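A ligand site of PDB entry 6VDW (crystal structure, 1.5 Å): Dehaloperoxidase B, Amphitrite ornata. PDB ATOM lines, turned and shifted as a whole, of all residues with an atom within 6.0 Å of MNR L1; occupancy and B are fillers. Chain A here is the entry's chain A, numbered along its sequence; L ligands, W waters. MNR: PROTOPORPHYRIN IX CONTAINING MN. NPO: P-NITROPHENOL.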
ATOM      1  N   PHE A  21       5.828 -18.032   6.345  1.00  0.00           N
ATOM      2  CA  PHE A  21       7.283 -18.000   6.396  1.00  0.00           C
ATOM      3  C   PHE A  21       7.884 -18.138   4.986  1.00  0.00           C
ATOM      4  O   PHE A  21       8.893 -17.488   4.688  1.00  0.00           O
ATOM      5  CB  PHE A  21       7.779 -19.136   7.294  1.00  0.00           C
ATOM      6  CG  PHE A  21       9.282 -19.151   7.527  1.00  0.00           C
ATOM      7  CD1 PHE A  21       9.917 -18.033   8.022  1.00  0.00           C
ATOM      8  CD2 PHE A  21      10.036 -20.233   7.180  1.00  0.00           C
ATOM      9  CE1 PHE A  21      11.327 -18.018   8.202  1.00  0.00           C
ATOM     10  CE2 PHE A  21      11.404 -20.235   7.394  1.00  0.00           C
ATOM     11  CZ  PHE A  21      12.049 -19.136   7.902  1.00  0.00           C
ATOM     12  N   PHE A  24       7.749 -14.759   3.465  1.00  0.00           N
ATOM     13  CA  PHE A  24       8.855 -13.967   4.005  1.00  0.00           C
ATOM     14  C   PHE A  24      10.174 -14.303   3.328  1.00  0.00           C
ATOM     15  O   PHE A  24      10.900 -13.390   2.869  1.00  0.00           O
ATOM     16  CB  PHE A  24       8.936 -14.231   5.513  1.00  0.00           C
ATOM     17  CG  PHE A  24      10.240 -13.833   6.160  1.00  0.00           C
ATOM     18  CD1 PHE A  24      10.510 -12.474   6.410  1.00  0.00           C
ATOM     19  CD2 PHE A  24      11.072 -14.811   6.623  1.00  0.00           C
ATOM     20  CE1 PHE A  24      11.716 -12.111   7.097  1.00  0.00           C
ATOM     21  CE2 PHE A  24      12.279 -14.462   7.314  1.00  0.00           C
ATOM     22  CZ  PHE A  24      12.535 -13.074   7.569  1.00  0.00           C
ATOM     23  N   GLU A  31      17.370 -12.992   3.810  1.00  0.00           N
ATOM     24  CA  GLU A  31      17.200 -13.474   5.182  1.00  0.00           C
ATOM     25  C   GLU A  31      17.690 -14.899   5.473  1.00  0.00           C
ATOM     26  O   GLU A  31      17.516 -15.397   6.546  1.00  0.00           O
ATOM     27  CB  GLU A  31      15.672 -13.268   5.557  1.00  0.00           C
ATOM     28  CG  GLU A  31      15.302 -11.768   5.644  1.00  0.00           C
ATOM     29  CD  GLU A  31      15.854 -11.114   6.930  1.00  0.00           C
ATOM     30  OE1 GLU A  31      16.580 -10.095   6.875  1.00  0.00           O
ATOM     31  OE2 GLU A  31      15.697 -11.731   7.989  1.00  0.00           O
ATOM     32  N   ASN A  34      20.224 -16.377   7.891  1.00  0.00           N
ATOM     33  CA  ASN A  34      19.962 -17.030   9.169  1.00  0.00           C
ATOM     34  C   ASN A  34      19.334 -18.402   9.035  1.00  0.00           C
ATOM     35  O   ASN A  34      19.025 -19.026  10.062  1.00  0.00           O
ATOM     36  CB  ASN A  34      19.051 -16.140  10.041  1.00  0.00           C
ATOM     37  CG  ASN A  34      19.770 -14.924  10.577  1.00  0.00           C
ATOM     38  OD1 ASN A  34      19.383 -13.793  10.301  1.00  0.00           O
ATOM     39  ND2 ASN A  34      20.826 -15.160  11.326  1.00  0.00           N
ATOM     40  N   PHE A  35      19.187 -18.905   7.818  1.00  0.00           N
ATOM     41  CA  PHE A  35      18.512 -20.198   7.578  1.00  0.00           C
ATOM     42  C   PHE A  35      19.292 -20.940   6.493  1.00  0.00           C
ATOM     43  O   PHE A  35      18.759 -21.289   5.427  1.00  0.00           O
ATOM     44  CB  PHE A  35      17.057 -19.968   7.131  1.00  0.00           C
ATOM     45  CG  PHE A  35      16.259 -19.173   8.111  1.00  0.00           C
ATOM     46  CD1 PHE A  35      15.887 -19.726   9.331  1.00  0.00           C
ATOM     47  CD2 PHE A  35      15.890 -17.882   7.852  1.00  0.00           C
ATOM     48  CE1 PHE A  35      15.214 -18.909  10.291  1.00  0.00           C
ATOM     49  CE2 PHE A  35      15.172 -17.104   8.789  1.00  0.00           C
ATOM     50  CZ  PHE A  35      14.833 -17.649  10.001  1.00  0.00           C
ATOM     51  N   TYR A  38      17.942 -23.929   4.519  1.00  0.00           N
ATOM     52  CA  TYR A  38      16.773 -23.813   3.655  1.00  0.00           C
ATOM     53  C   TYR A  38      17.156 -23.284   2.271  1.00  0.00           C
ATOM     54  O   TYR A  38      16.282 -23.072   1.418  1.00  0.00           O
ATOM     55  CB  TYR A  38      15.680 -22.911   4.349  1.00  0.00           C
ATOM     56  CG  TYR A  38      15.157 -23.388   5.727  1.00  0.00           C
ATOM     57  CD1 TYR A  38      15.238 -24.732   6.088  1.00  0.00           C
ATOM     58  CD2 TYR A  38      14.633 -22.478   6.622  1.00  0.00           C
ATOM     59  CE1 TYR A  38      14.799 -25.148   7.328  1.00  0.00           C
ATOM     60  CE2 TYR A  38      14.201 -22.886   7.858  1.00  0.00           C
ATOM     61  CZ  TYR A  38      14.259 -24.227   8.181  1.00  0.00           C
ATOM     62  OH  TYR A  38      13.857 -24.629   9.462  1.00  0.00           O
ATOM     63  N   ASP A  54       8.548 -28.490  11.304  1.00  0.00           N
ATOM     64  CA  ASP A  54       8.402 -28.499  12.747  1.00  0.00           C
ATOM     65  C   ASP A  54       8.814 -27.176  13.358  1.00  0.00           C
ATOM     66  O   ASP A  54       8.140 -26.654  14.248  1.00  0.00           O
ATOM     67  CB  ASP A  54       9.222 -29.638  13.360  1.00  0.00           C
ATOM     68  CG  ASP A  54       8.659 -31.003  13.022  1.00  0.00           C
ATOM     69  OD1 ASP A  54       7.476 -31.114  12.665  1.00  0.00           O
ATOM     70  OD2 ASP A  54       9.440 -31.993  13.098  1.00  0.00           O
ATOM     71  N   HIS A  55       9.936 -26.602  12.889  1.00  0.00           N
ATOM     72  CA  HIS A  55      10.361 -25.341  13.482  1.00  0.00           C
ATOM     73  C   HIS A  55       9.422 -24.224  13.088  1.00  0.00           C
ATOM     74  O   HIS A  55       9.115 -23.372  13.934  1.00  0.00           O
ATOM     75  CB  HIS A  55      11.753 -24.926  13.033  1.00  0.00           C
ATOM     76  CG  HIS A  55      12.841 -25.775  13.601  1.00  0.00           C
ATOM     77  ND1 HIS A  55      14.046 -25.239  14.010  1.00  0.00           N
ATOM     78  CD2 HIS A  55      12.895 -27.107  13.869  1.00  0.00           C
ATOM     79  CE1 HIS A  55      14.813 -26.215  14.475  1.00  0.00           C
ATOM     80  NE2 HIS A  55      14.137 -27.349  14.435  1.00  0.00           N
ATOM     81  N   THR A  56       8.941 -24.183  11.834  1.00  0.00           N
ATOM     82  CA  THR A  56       8.042 -23.081  11.457  1.00  0.00           C
ATOM     83  C   THR A  56       6.761 -23.171  12.261  1.00  0.00           C
ATOM     84  O   THR A  56       6.221 -22.157  12.721  1.00  0.00           O
ATOM     85  CB  THR A  56       7.738 -23.120   9.958  1.00  0.00           C
ATOM     86  OG1 THR A  56       8.987 -23.033   9.245  1.00  0.00           O
ATOM     87  CG2 THR A  56       6.881 -21.970   9.549  1.00  0.00           C
ATOM     88  N   LYS A  58       6.340 -24.510  15.237  1.00  0.00           N
ATOM     89  CA  LYS A  58       6.622 -24.119  16.626  1.00  0.00           C
ATOM     90  C   LYS A  58       6.822 -22.615  16.778  1.00  0.00           C
ATOM     91  O   LYS A  58       6.375 -22.040  17.768  1.00  0.00           O
ATOM     92  CB  LYS A  58       7.831 -24.889  17.170  1.00  0.00           C
ATOM     93  CG  LYS A  58       7.443 -26.362  17.511  1.00  0.00           C
ATOM     94  CD  LYS A  58       8.680 -27.151  17.875  1.00  0.00           C
ATOM     95  CE  LYS A  58       8.351 -28.567  18.368  1.00  0.00           C
ATOM     96  NZ  LYS A  58       9.630 -29.440  18.462  1.00  0.00           N
ATOM     97  N   VAL A  59       7.466 -21.952  15.811  1.00  0.00           N
ATOM     98  CA  VAL A  59       7.534 -20.484  15.809  1.00  0.00           C
ATOM     99  C   VAL A  59       6.145 -19.887  15.853  1.00  0.00           C
ATOM    100  O   VAL A  59       5.845 -18.966  16.647  1.00  0.00           O
ATOM    101  CB  VAL A  59       8.308 -20.003  14.560  1.00  0.00           C
ATOM    102  CG1 VAL A  59       8.030 -18.484  14.328  1.00  0.00           C
ATOM    103  CG2 VAL A  59       9.792 -20.318  14.676  1.00  0.00           C
ATOM    104  N   PHE A  60       5.270 -20.363  14.962  1.00  0.00           N
ATOM    105  CA  PHE A  60       3.928 -19.774  14.924  1.00  0.00           C
ATOM    106  C   PHE A  60       3.057 -20.187  16.101  1.00  0.00           C
ATOM    107  O   PHE A  60       2.178 -19.399  16.519  1.00  0.00           O
ATOM    108  CB  PHE A  60       3.241 -20.081  13.582  1.00  0.00           C
ATOM    109  CG  PHE A  60       3.670 -19.138  12.500  1.00  0.00           C
ATOM    110  CD1 PHE A  60       4.967 -19.156  11.995  1.00  0.00           C
ATOM    111  CD2 PHE A  60       2.783 -18.159  12.090  1.00  0.00           C
ATOM    112  CE1 PHE A  60       5.360 -18.219  11.016  1.00  0.00           C
ATOM    113  CE2 PHE A  60       3.173 -17.242  11.095  1.00  0.00           C
ATOM    114  CZ  PHE A  60       4.477 -17.252  10.587  1.00  0.00           C
ATOM    115  N   LEU A  62       4.094 -20.300  19.138  1.00  0.00           N
ATOM    116  CA  LEU A  62       4.435 -19.290  20.141  1.00  0.00           C
ATOM    117  C   LEU A  62       3.976 -17.911  19.708  1.00  0.00           C
ATOM    118  O   LEU A  62       3.473 -17.148  20.533  1.00  0.00           O
ATOM    119  CB  LEU A  62       5.946 -19.337  20.444  1.00  0.00           C
ATOM    120  CG  LEU A  62       6.367 -18.309  21.521  1.00  0.00           C
ATOM    121  CD1 LEU A  62       5.652 -18.611  22.880  1.00  0.00           C
ATOM    122  CD2 LEU A  62       7.884 -18.477  21.686  1.00  0.00           C
ATOM    123  N   MET A  63       4.086 -17.587  18.400  1.00  0.00           N
ATOM    124  CA  MET A  63       3.604 -16.297  17.943  1.00  0.00           C
ATOM    125  C   MET A  63       2.122 -16.131  18.287  1.00  0.00           C
ATOM    126  O   MET A  63       1.714 -15.044  18.701  1.00  0.00           O
ATOM    127  CB  MET A  63       3.840 -16.140  16.443  1.00  0.00           C
ATOM    128  CG  MET A  63       3.467 -14.722  16.015  1.00  0.00           C
ATOM    129  SD  MET A  63       3.242 -14.561  14.174  1.00  0.00           S
ATOM    130  CE  MET A  63       4.922 -14.964  13.590  1.00  0.00           C
ATOM    131  N   VAL A  66       1.799 -15.299  21.996  1.00  0.00           N
ATOM    132  CA  VAL A  66       2.152 -13.920  22.267  1.00  0.00           C
ATOM    133  C   VAL A  66       1.029 -12.987  21.821  1.00  0.00           C
ATOM    134  O   VAL A  66       0.678 -12.037  22.513  1.00  0.00           O
ATOM    135  CB  VAL A  66       3.486 -13.583  21.555  1.00  0.00           C
ATOM    136  CG1 VAL A  66       3.871 -12.139  21.718  1.00  0.00           C
ATOM    137  CG2 VAL A  66       4.621 -14.510  22.166  1.00  0.00           C
ATOM    138  N   LEU A  83      11.625 -13.485  23.847  1.00  0.00           N
ATOM    139  CA  LEU A  83      12.062 -13.490  22.445  1.00  0.00           C
ATOM    140  C   LEU A  83      13.431 -12.834  22.242  1.00  0.00           C
ATOM    141  O   LEU A  83      14.183 -13.251  21.362  1.00  0.00           O
ATOM    142  CB  LEU A  83      10.999 -12.791  21.617  1.00  0.00           C
ATOM    143  CG  LEU A  83       9.646 -13.518  21.498  1.00  0.00           C
ATOM    144  CD1 LEU A  83       8.609 -12.491  20.895  1.00  0.00           C
ATOM    145  CD2 LEU A  83       9.789 -14.717  20.524  1.00  0.00           C
ATOM    146  N   MET A  86      16.126 -15.616  24.026  1.00  0.00           N
ATOM    147  CA  MET A  86      16.314 -17.003  23.608  1.00  0.00           C
ATOM    148  C   MET A  86      17.587 -17.136  22.791  1.00  0.00           C
ATOM    149  O   MET A  86      17.899 -16.272  21.963  1.00  0.00           O
ATOM    150  CB  MET A  86      15.087 -17.547  22.815  1.00  0.00           C
ATOM    151  CG  MET A  86      14.285 -16.639  21.965  1.00  0.00           C
ATOM    152  SD  MET A  86      12.665 -17.481  21.656  1.00  0.00           S
ATOM    153  CE  MET A  86      13.172 -18.697  20.445  1.00  0.00           C
ATOM    154  N   GLN A  88      18.368 -19.070  20.431  1.00  0.00           N
ATOM    155  CA  GLN A  88      18.084 -19.190  19.013  1.00  0.00           C
ATOM    156  C   GLN A  88      18.000 -17.830  18.332  1.00  0.00           C
ATOM    157  O   GLN A  88      18.081 -17.736  17.112  1.00  0.00           O
ATOM    158  CB  GLN A  88      16.766 -19.968  18.848  1.00  0.00           C
ATOM    159  CG  GLN A  88      16.728 -21.348  19.527  1.00  0.00           C
ATOM    160  CD  GLN A  88      16.269 -21.350  20.998  1.00  0.00           C
ATOM    161  OE1 GLN A  88      16.358 -20.351  21.695  1.00  0.00           O
ATOM    162  NE2 GLN A  88      15.799 -22.502  21.459  1.00  0.00           N
ATOM    163  N   HIS A  89      17.822 -16.755  19.115  1.00  0.00           N
ATOM    164  CA  HIS A  89      17.672 -15.421  18.560  1.00  0.00           C
ATOM    165  C   HIS A  89      18.918 -14.572  18.741  1.00  0.00           C
ATOM    166  O   HIS A  89      18.891 -13.377  18.440  1.00  0.00           O
ATOM    167  CB  HIS A  89      16.455 -14.725  19.175  1.00  0.00           C
ATOM    168  CG  HIS A  89      15.178 -15.315  18.688  1.00  0.00           C
ATOM    169  ND1 HIS A  89      13.966 -14.908  19.200  1.00  0.00           N
ATOM    170  CD2 HIS A  89      14.911 -16.209  17.714  1.00  0.00           C
ATOM    171  CE1 HIS A  89      12.987 -15.571  18.600  1.00  0.00           C
ATOM    172  NE2 HIS A  89      13.536 -16.361  17.679  1.00  0.00           N
ATOM    173  N   LEU A  92      20.095 -11.828  16.107  1.00  0.00           N
ATOM    174  CA  LEU A  92      19.028 -11.193  15.349  1.00  0.00           C
ATOM    175  C   LEU A  92      18.889  -9.719  15.745  1.00  0.00           C
ATOM    176  O   LEU A  92      19.296  -9.302  16.839  1.00  0.00           O
ATOM    177  CB  LEU A  92      17.692 -11.916  15.594  1.00  0.00           C
ATOM    178  CG  LEU A  92      17.555 -13.347  15.032  1.00  0.00           C
ATOM    179  CD1 LEU A  92      16.147 -13.893  15.308  1.00  0.00           C
ATOM    180  CD2 LEU A  92      17.961 -13.348  13.477  1.00  0.00           C
ATOM    181  N   ASN A  96      14.787  -8.012  11.407  1.00  0.00           N
ATOM    182  CA  ASN A  96      14.406  -9.383  11.003  1.00  0.00           C
ATOM    183  C   ASN A  96      12.925  -9.600  11.312  1.00  0.00           C
ATOM    184  O   ASN A  96      12.171 -10.164  10.494  1.00  0.00           O
ATOM    185  CB  ASN A  96      15.241 -10.424  11.745  1.00  0.00           C
ATOM    186  CG  ASN A  96      16.705 -10.335  11.432  1.00  0.00           C
ATOM    187  OD1 ASN A  96      17.524 -10.136  12.344  1.00  0.00           O
ATOM    188  ND2 ASN A  96      17.075 -10.596  10.175  1.00  0.00           N
ATOM    189  N   PHE A  97      12.487  -9.116  12.492  1.00  0.00           N
ATOM    190  CA  PHE A  97      11.077  -9.231  12.886  1.00  0.00           C
ATOM    191  C   PHE A  97      10.163  -8.314  12.087  1.00  0.00           C
ATOM    192  O   PHE A  97       9.062  -8.727  11.719  1.00  0.00           O
ATOM    193  CB  PHE A  97      10.951  -8.970  14.411  1.00  0.00           C
ATOM    194  CG  PHE A  97      11.566 -10.063  15.232  1.00  0.00           C
ATOM    195  CD1 PHE A  97      12.948 -10.143  15.390  1.00  0.00           C
ATOM    196  CD2 PHE A  97      10.792 -11.072  15.821  1.00  0.00           C
ATOM    197  CE1 PHE A  97      13.565 -11.145  16.134  1.00  0.00           C
ATOM    198  CE2 PHE A  97      11.396 -12.088  16.602  1.00  0.00           C
ATOM    199  CZ  PHE A  97      12.811 -12.131  16.723  1.00  0.00           C
ATOM    200  N   LEU A 100       9.455 -10.076   8.796  1.00  0.00           N
ATOM    201  CA  LEU A 100       8.519 -11.182   8.906  1.00  0.00           C
ATOM    202  C   LEU A 100       7.097 -10.653   8.953  1.00  0.00           C
ATOM    203  O   LEU A 100       6.193 -11.201   8.287  1.00  0.00           O
ATOM    204  CB  LEU A 100       8.827 -12.035  10.135  1.00  0.00           C
ATOM    205  CG  LEU A 100       7.818 -13.158  10.411  1.00  0.00           C
ATOM    206  CD1 LEU A 100       7.805 -14.192   9.276  1.00  0.00           C
ATOM    207  CD2 LEU A 100       8.240 -13.801  11.709  1.00  0.00           C
ATOM    208  N   PHE A 101       6.865  -9.593   9.750  1.00  0.00           N
ATOM    209  CA  PHE A 101       5.498  -9.075   9.852  1.00  0.00           C
ATOM    210  C   PHE A 101       5.061  -8.310   8.609  1.00  0.00           C
ATOM    211  O   PHE A 101       3.871  -8.320   8.310  1.00  0.00           O
ATOM    212  CB  PHE A 101       5.301  -8.261  11.150  1.00  0.00           C
ATOM    213  CG  PHE A 101       5.123  -9.188  12.326  1.00  0.00           C
ATOM    214  CD1 PHE A 101       3.878  -9.683  12.630  1.00  0.00           C
ATOM    215  CD2 PHE A 101       6.223  -9.650  13.031  1.00  0.00           C
ATOM    216  CE1 PHE A 101       3.761 -10.636  13.643  1.00  0.00           C
ATOM    217  CE2 PHE A 101       6.119 -10.589  14.037  1.00  0.00           C
ATOM    218  CZ  PHE A 101       4.882 -11.088  14.351  1.00  0.00           C
ATOM    219  N   PHE A 123       0.441  -4.990  15.501  1.00  0.00           N
ATOM    220  CA  PHE A 123       1.116  -5.921  16.362  1.00  0.00           C
ATOM    221  C   PHE A 123       2.574  -6.070  15.975  1.00  0.00           C
ATOM    222  O   PHE A 123       3.448  -6.161  16.848  1.00  0.00           O
ATOM    223  CB  PHE A 123       0.363  -7.298  16.254  1.00  0.00           C
ATOM    224  CG  PHE A 123       0.996  -8.435  17.009  1.00  0.00           C
ATOM    225  CD1 PHE A 123       1.045  -8.404  18.392  1.00  0.00           C
ATOM    226  CD2 PHE A 123       1.502  -9.569  16.367  1.00  0.00           C
ATOM    227  CE1 PHE A 123       1.631  -9.442  19.120  1.00  0.00           C
ATOM    228  CE2 PHE A 123       2.118 -10.634  17.095  1.00  0.00           C
ATOM    229  CZ  PHE A 123       2.137 -10.577  18.477  1.00  0.00           C
ATOM    230  N   LEU A 127       5.410  -5.208  18.577  1.00  0.00           N
ATOM    231  CA  LEU A 127       6.384  -6.224  18.948  1.00  0.00           C
ATOM    232  C   LEU A 127       7.792  -5.691  18.739  1.00  0.00           C
ATOM    233  O   LEU A 127       8.646  -5.881  19.600  1.00  0.00           O
ATOM    234  CB  LEU A 127       6.154  -7.558  18.136  1.00  0.00           C
ATOM    235  CG  LEU A 127       7.047  -8.693  18.649  1.00  0.00           C
ATOM    236  CD1 LEU A 127       6.962  -9.057  20.142  1.00  0.00           C
ATOM    237  CD2 LEU A 127       6.692  -9.943  17.808  1.00  0.00           C
HETATM  238  CHA MNR L   1      13.797 -20.453  16.584  1.00  0.00           C
HETATM  239  CHB MNR L   1       9.848 -18.284  18.013  1.00  0.00           C
HETATM  240  CHC MNR L   1      10.697 -14.747  14.833  1.00  0.00           C
HETATM  241  CHD MNR L   1      15.040 -16.773  13.656  1.00  0.00           C
HETATM  242  C1A MNR L   1      12.503 -20.288  17.239  1.00  0.00           C
HETATM  243  C2A MNR L   1      11.881 -21.163  17.994  1.00  0.00           C
HETATM  244  C3A MNR L   1      10.687 -20.477  18.438  1.00  0.00           C
HETATM  245  C4A MNR L   1      10.865 -19.240  17.812  1.00  0.00           C
HETATM  246  CMA MNR L   1       9.717 -21.168  19.298  1.00  0.00           C
HETATM  247  CAA MNR L   1      12.276 -22.649  18.341  1.00  0.00           C
HETATM  248  CBA MNR L   1      11.909 -23.623  17.049  1.00  0.00           C
HETATM  249  CGA MNR L   1      12.231 -25.058  17.365  1.00  0.00           C
HETATM  250  O1A MNR L   1      13.474 -25.291  17.729  1.00  0.00           O
HETATM  251  O2A MNR L   1      11.626 -25.807  16.778  1.00  0.00           O
HETATM  252  C1B MNR L   1       9.567 -17.151  17.347  1.00  0.00           C
HETATM  253  C2B MNR L   1       8.647 -16.170  17.227  1.00  0.00           C
HETATM  254  C3B MNR L   1       8.788 -15.079  16.289  1.00  0.00           C
HETATM  255  C4B MNR L   1      10.027 -15.409  15.783  1.00  0.00           C
HETATM  256  CMB MNR L   1       7.305 -16.371  18.167  1.00  0.00           C
HETATM  257  CAB MNR L   1       8.042 -14.117  15.992  1.00  0.00           C
HETATM  258  CBB MNR L   1       7.148 -13.317  16.821  1.00  0.00           C
HETATM  259  C1C MNR L   1      11.909 -15.007  14.146  1.00  0.00           C
HETATM  260  C2C MNR L   1      12.389 -14.063  13.106  1.00  0.00           C
HETATM  261  C3C MNR L   1      13.689 -14.774  12.784  1.00  0.00           C
HETATM  262  C4C MNR L   1      13.827 -15.943  13.656  1.00  0.00           C
HETATM  263  CMC MNR L   1      11.833 -12.922  12.576  1.00  0.00           C
HETATM  264  CAC MNR L   1      14.624 -14.387  11.833  1.00  0.00           C
HETATM  265  CBC MNR L   1      14.363 -13.817  10.596  1.00  0.00           C
HETATM  266  C1D MNR L   1      15.124 -17.919  14.344  1.00  0.00           C
HETATM  267  C2D MNR L   1      16.026 -18.910  14.343  1.00  0.00           C
HETATM  268  C3D MNR L   1      15.886 -19.858  14.970  1.00  0.00           C
HETATM  269  C4D MNR L   1      14.519 -19.727  15.753  1.00  0.00           C
HETATM  270  CMD MNR L   1      17.431 -18.684  13.363  1.00  0.00           C
HETATM  271  CAD MNR L   1      16.627 -21.310  15.355  1.00  0.00           C
HETATM  272  CBD MNR L   1      17.128 -21.873  14.215  1.00  0.00           C
HETATM  273  CGD MNR L   1      15.883 -22.548  13.344  1.00  0.00           C
HETATM  274  O1D MNR L   1      15.764 -22.268  12.209  1.00  0.00           O
HETATM  275  O2D MNR L   1      15.030 -22.812  14.258  1.00  0.00           O
HETATM  276 MN   MNR L   1      12.462 -17.448  15.989  1.00  0.00          MN
HETATM  277  NA  MNR L   1      11.935 -19.101  17.079  1.00  0.00           N
HETATM  278  NB  MNR L   1      10.695 -16.635  16.313  1.00  0.00           N
HETATM  279  NC  MNR L   1      12.764 -16.144  14.551  1.00  0.00           N
HETATM  280  ND  MNR L   1      14.185 -18.436  15.214  1.00  0.00           N
HETATM  281  C1  NPO L   2      10.864 -19.275  11.438  1.00  0.00           C
HETATM  282  C2  NPO L   2      12.088 -19.196  12.155  1.00  0.00           C
HETATM  283  C3  NPO L   2      12.871 -20.322  12.182  1.00  0.00           C
HETATM  284  C4  NPO L   2      12.577 -21.512  11.471  1.00  0.00           C
HETATM  285  C5  NPO L   2      11.406 -21.545  10.774  1.00  0.00           C
HETATM  286  C6  NPO L   2      10.599 -20.461  10.762  1.00  0.00           C
HETATM  287  OH  NPO L   2      13.401 -22.657  11.411  1.00  0.00           O
HETATM  288  N1  NPO L   2      10.019 -18.145  11.359  1.00  0.00           N
HETATM  289  O2  NPO L   2      10.501 -16.890  11.700  1.00  0.00           O
HETATM  290  O3  NPO L   2       8.912 -18.171  10.932  1.00  0.00           O
HETATM  291  O   HOH W   1      11.988 -28.302  16.935  1.00  0.00           O
HETATM  292  O   HOH W   2      16.949 -13.836   8.646  1.00  0.00           O
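Phe 24 touches MNR L1.
OE2 of Glu 31 touches CBC of MNR L1 (3.6 Å).
O of Asn 34 touches CMD of MNR L1 (3.7 Å).
Phe 35 touches MNR L1.
Lys 58 touches MNR L1.
O of Val 59 touches CMB of MNR L1 (3.3 Å).
C of Leu 62 touches CMB of MNR L1 (3.98 Å).
N of Met 63 touches CMB of MNR L1 (3.4 Å).
Leu 83 touches MNR L1.
CE of Met 86 touches C4A of MNR L1 (3.5 Å).
Gln 88 touches MNR L1 (O to C2D, 3.6 Å).
Leu 92 touches MNR L1.
Asn 96 touches MNR L1 (O to CMC, 3.5 Å).
Phe 97 touches MNR L1.
Leu 100 touches MNR L1.
Leu 127 touches MNR L1 (CD2 to CBB, 3.5 Å).
Hydrophobic or aromatic side chains that line MNR L1: Phe 24, Phe 35, His 55, Val 59, Leu 62, Met 63, Leu 83, Met 86, His 89, Leu 92, Phe 97, Leu 100 and Leu 127.
18 residues have an atom within 4 Å of MNR L1: Phe 24, Glu 31, Asn 34, Phe 35, His 55, Lys 58, Val 59, Leu 62, Met 63, Leu 83, Met 86, Gln 88, His 89, Leu 92, Asn 96, Phe 97, Leu 100 and Leu 127.
The nearest printed residue that does not touch MNR L1 is Phe 101 (4.03 Å).
The side-chain sulfur of Met 86 sits close to a ring nitrogen (ND1) of His 89 (3.8 Å).
A ring nitrogen (ND1) of His 89 is in hydrogen-bond range of the backbone carbonyl oxygen (O) of Leu 83, 2.7 Å away.
OE2 of Glu 31 sits at hydrogen-bond distance from ND2 of Asn 96 (2.8 Å).
A manganese atom (MN) of MNR L1 is bound by a ring nitrogen (NE2) of His 89, 2.3 Å away.
A ring nitrogen (ND1) of His 55 lies within hydrogen-bond range of an oxygen (O2D) of MNR L1, 2.6 Å away.
The side-chain hydroxyl of Tyr 38 is in hydrogen-bond range of an oxygen (OH) of NPO L2, at 2.8 Å.
Water W1 lies within hydrogen-bond range of an oxygen (O2A) of MNR L1 (2.5 Å), the side-chain amino group (NZ) of Lys 58 (3.0 Å) and a ring nitrogen (NE2) of His 55 (3.4 Å).
Water W2 bridges the side-chain carboxylate (OE2) of Glu 31 (2.5 Å) and the side-chain amide oxygen (OD1) of Asn 34 (2.9 Å).
OH of NPO L2 sits at hydrogen-bond distance from O1D of MNR L1, at 2.5 Å.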
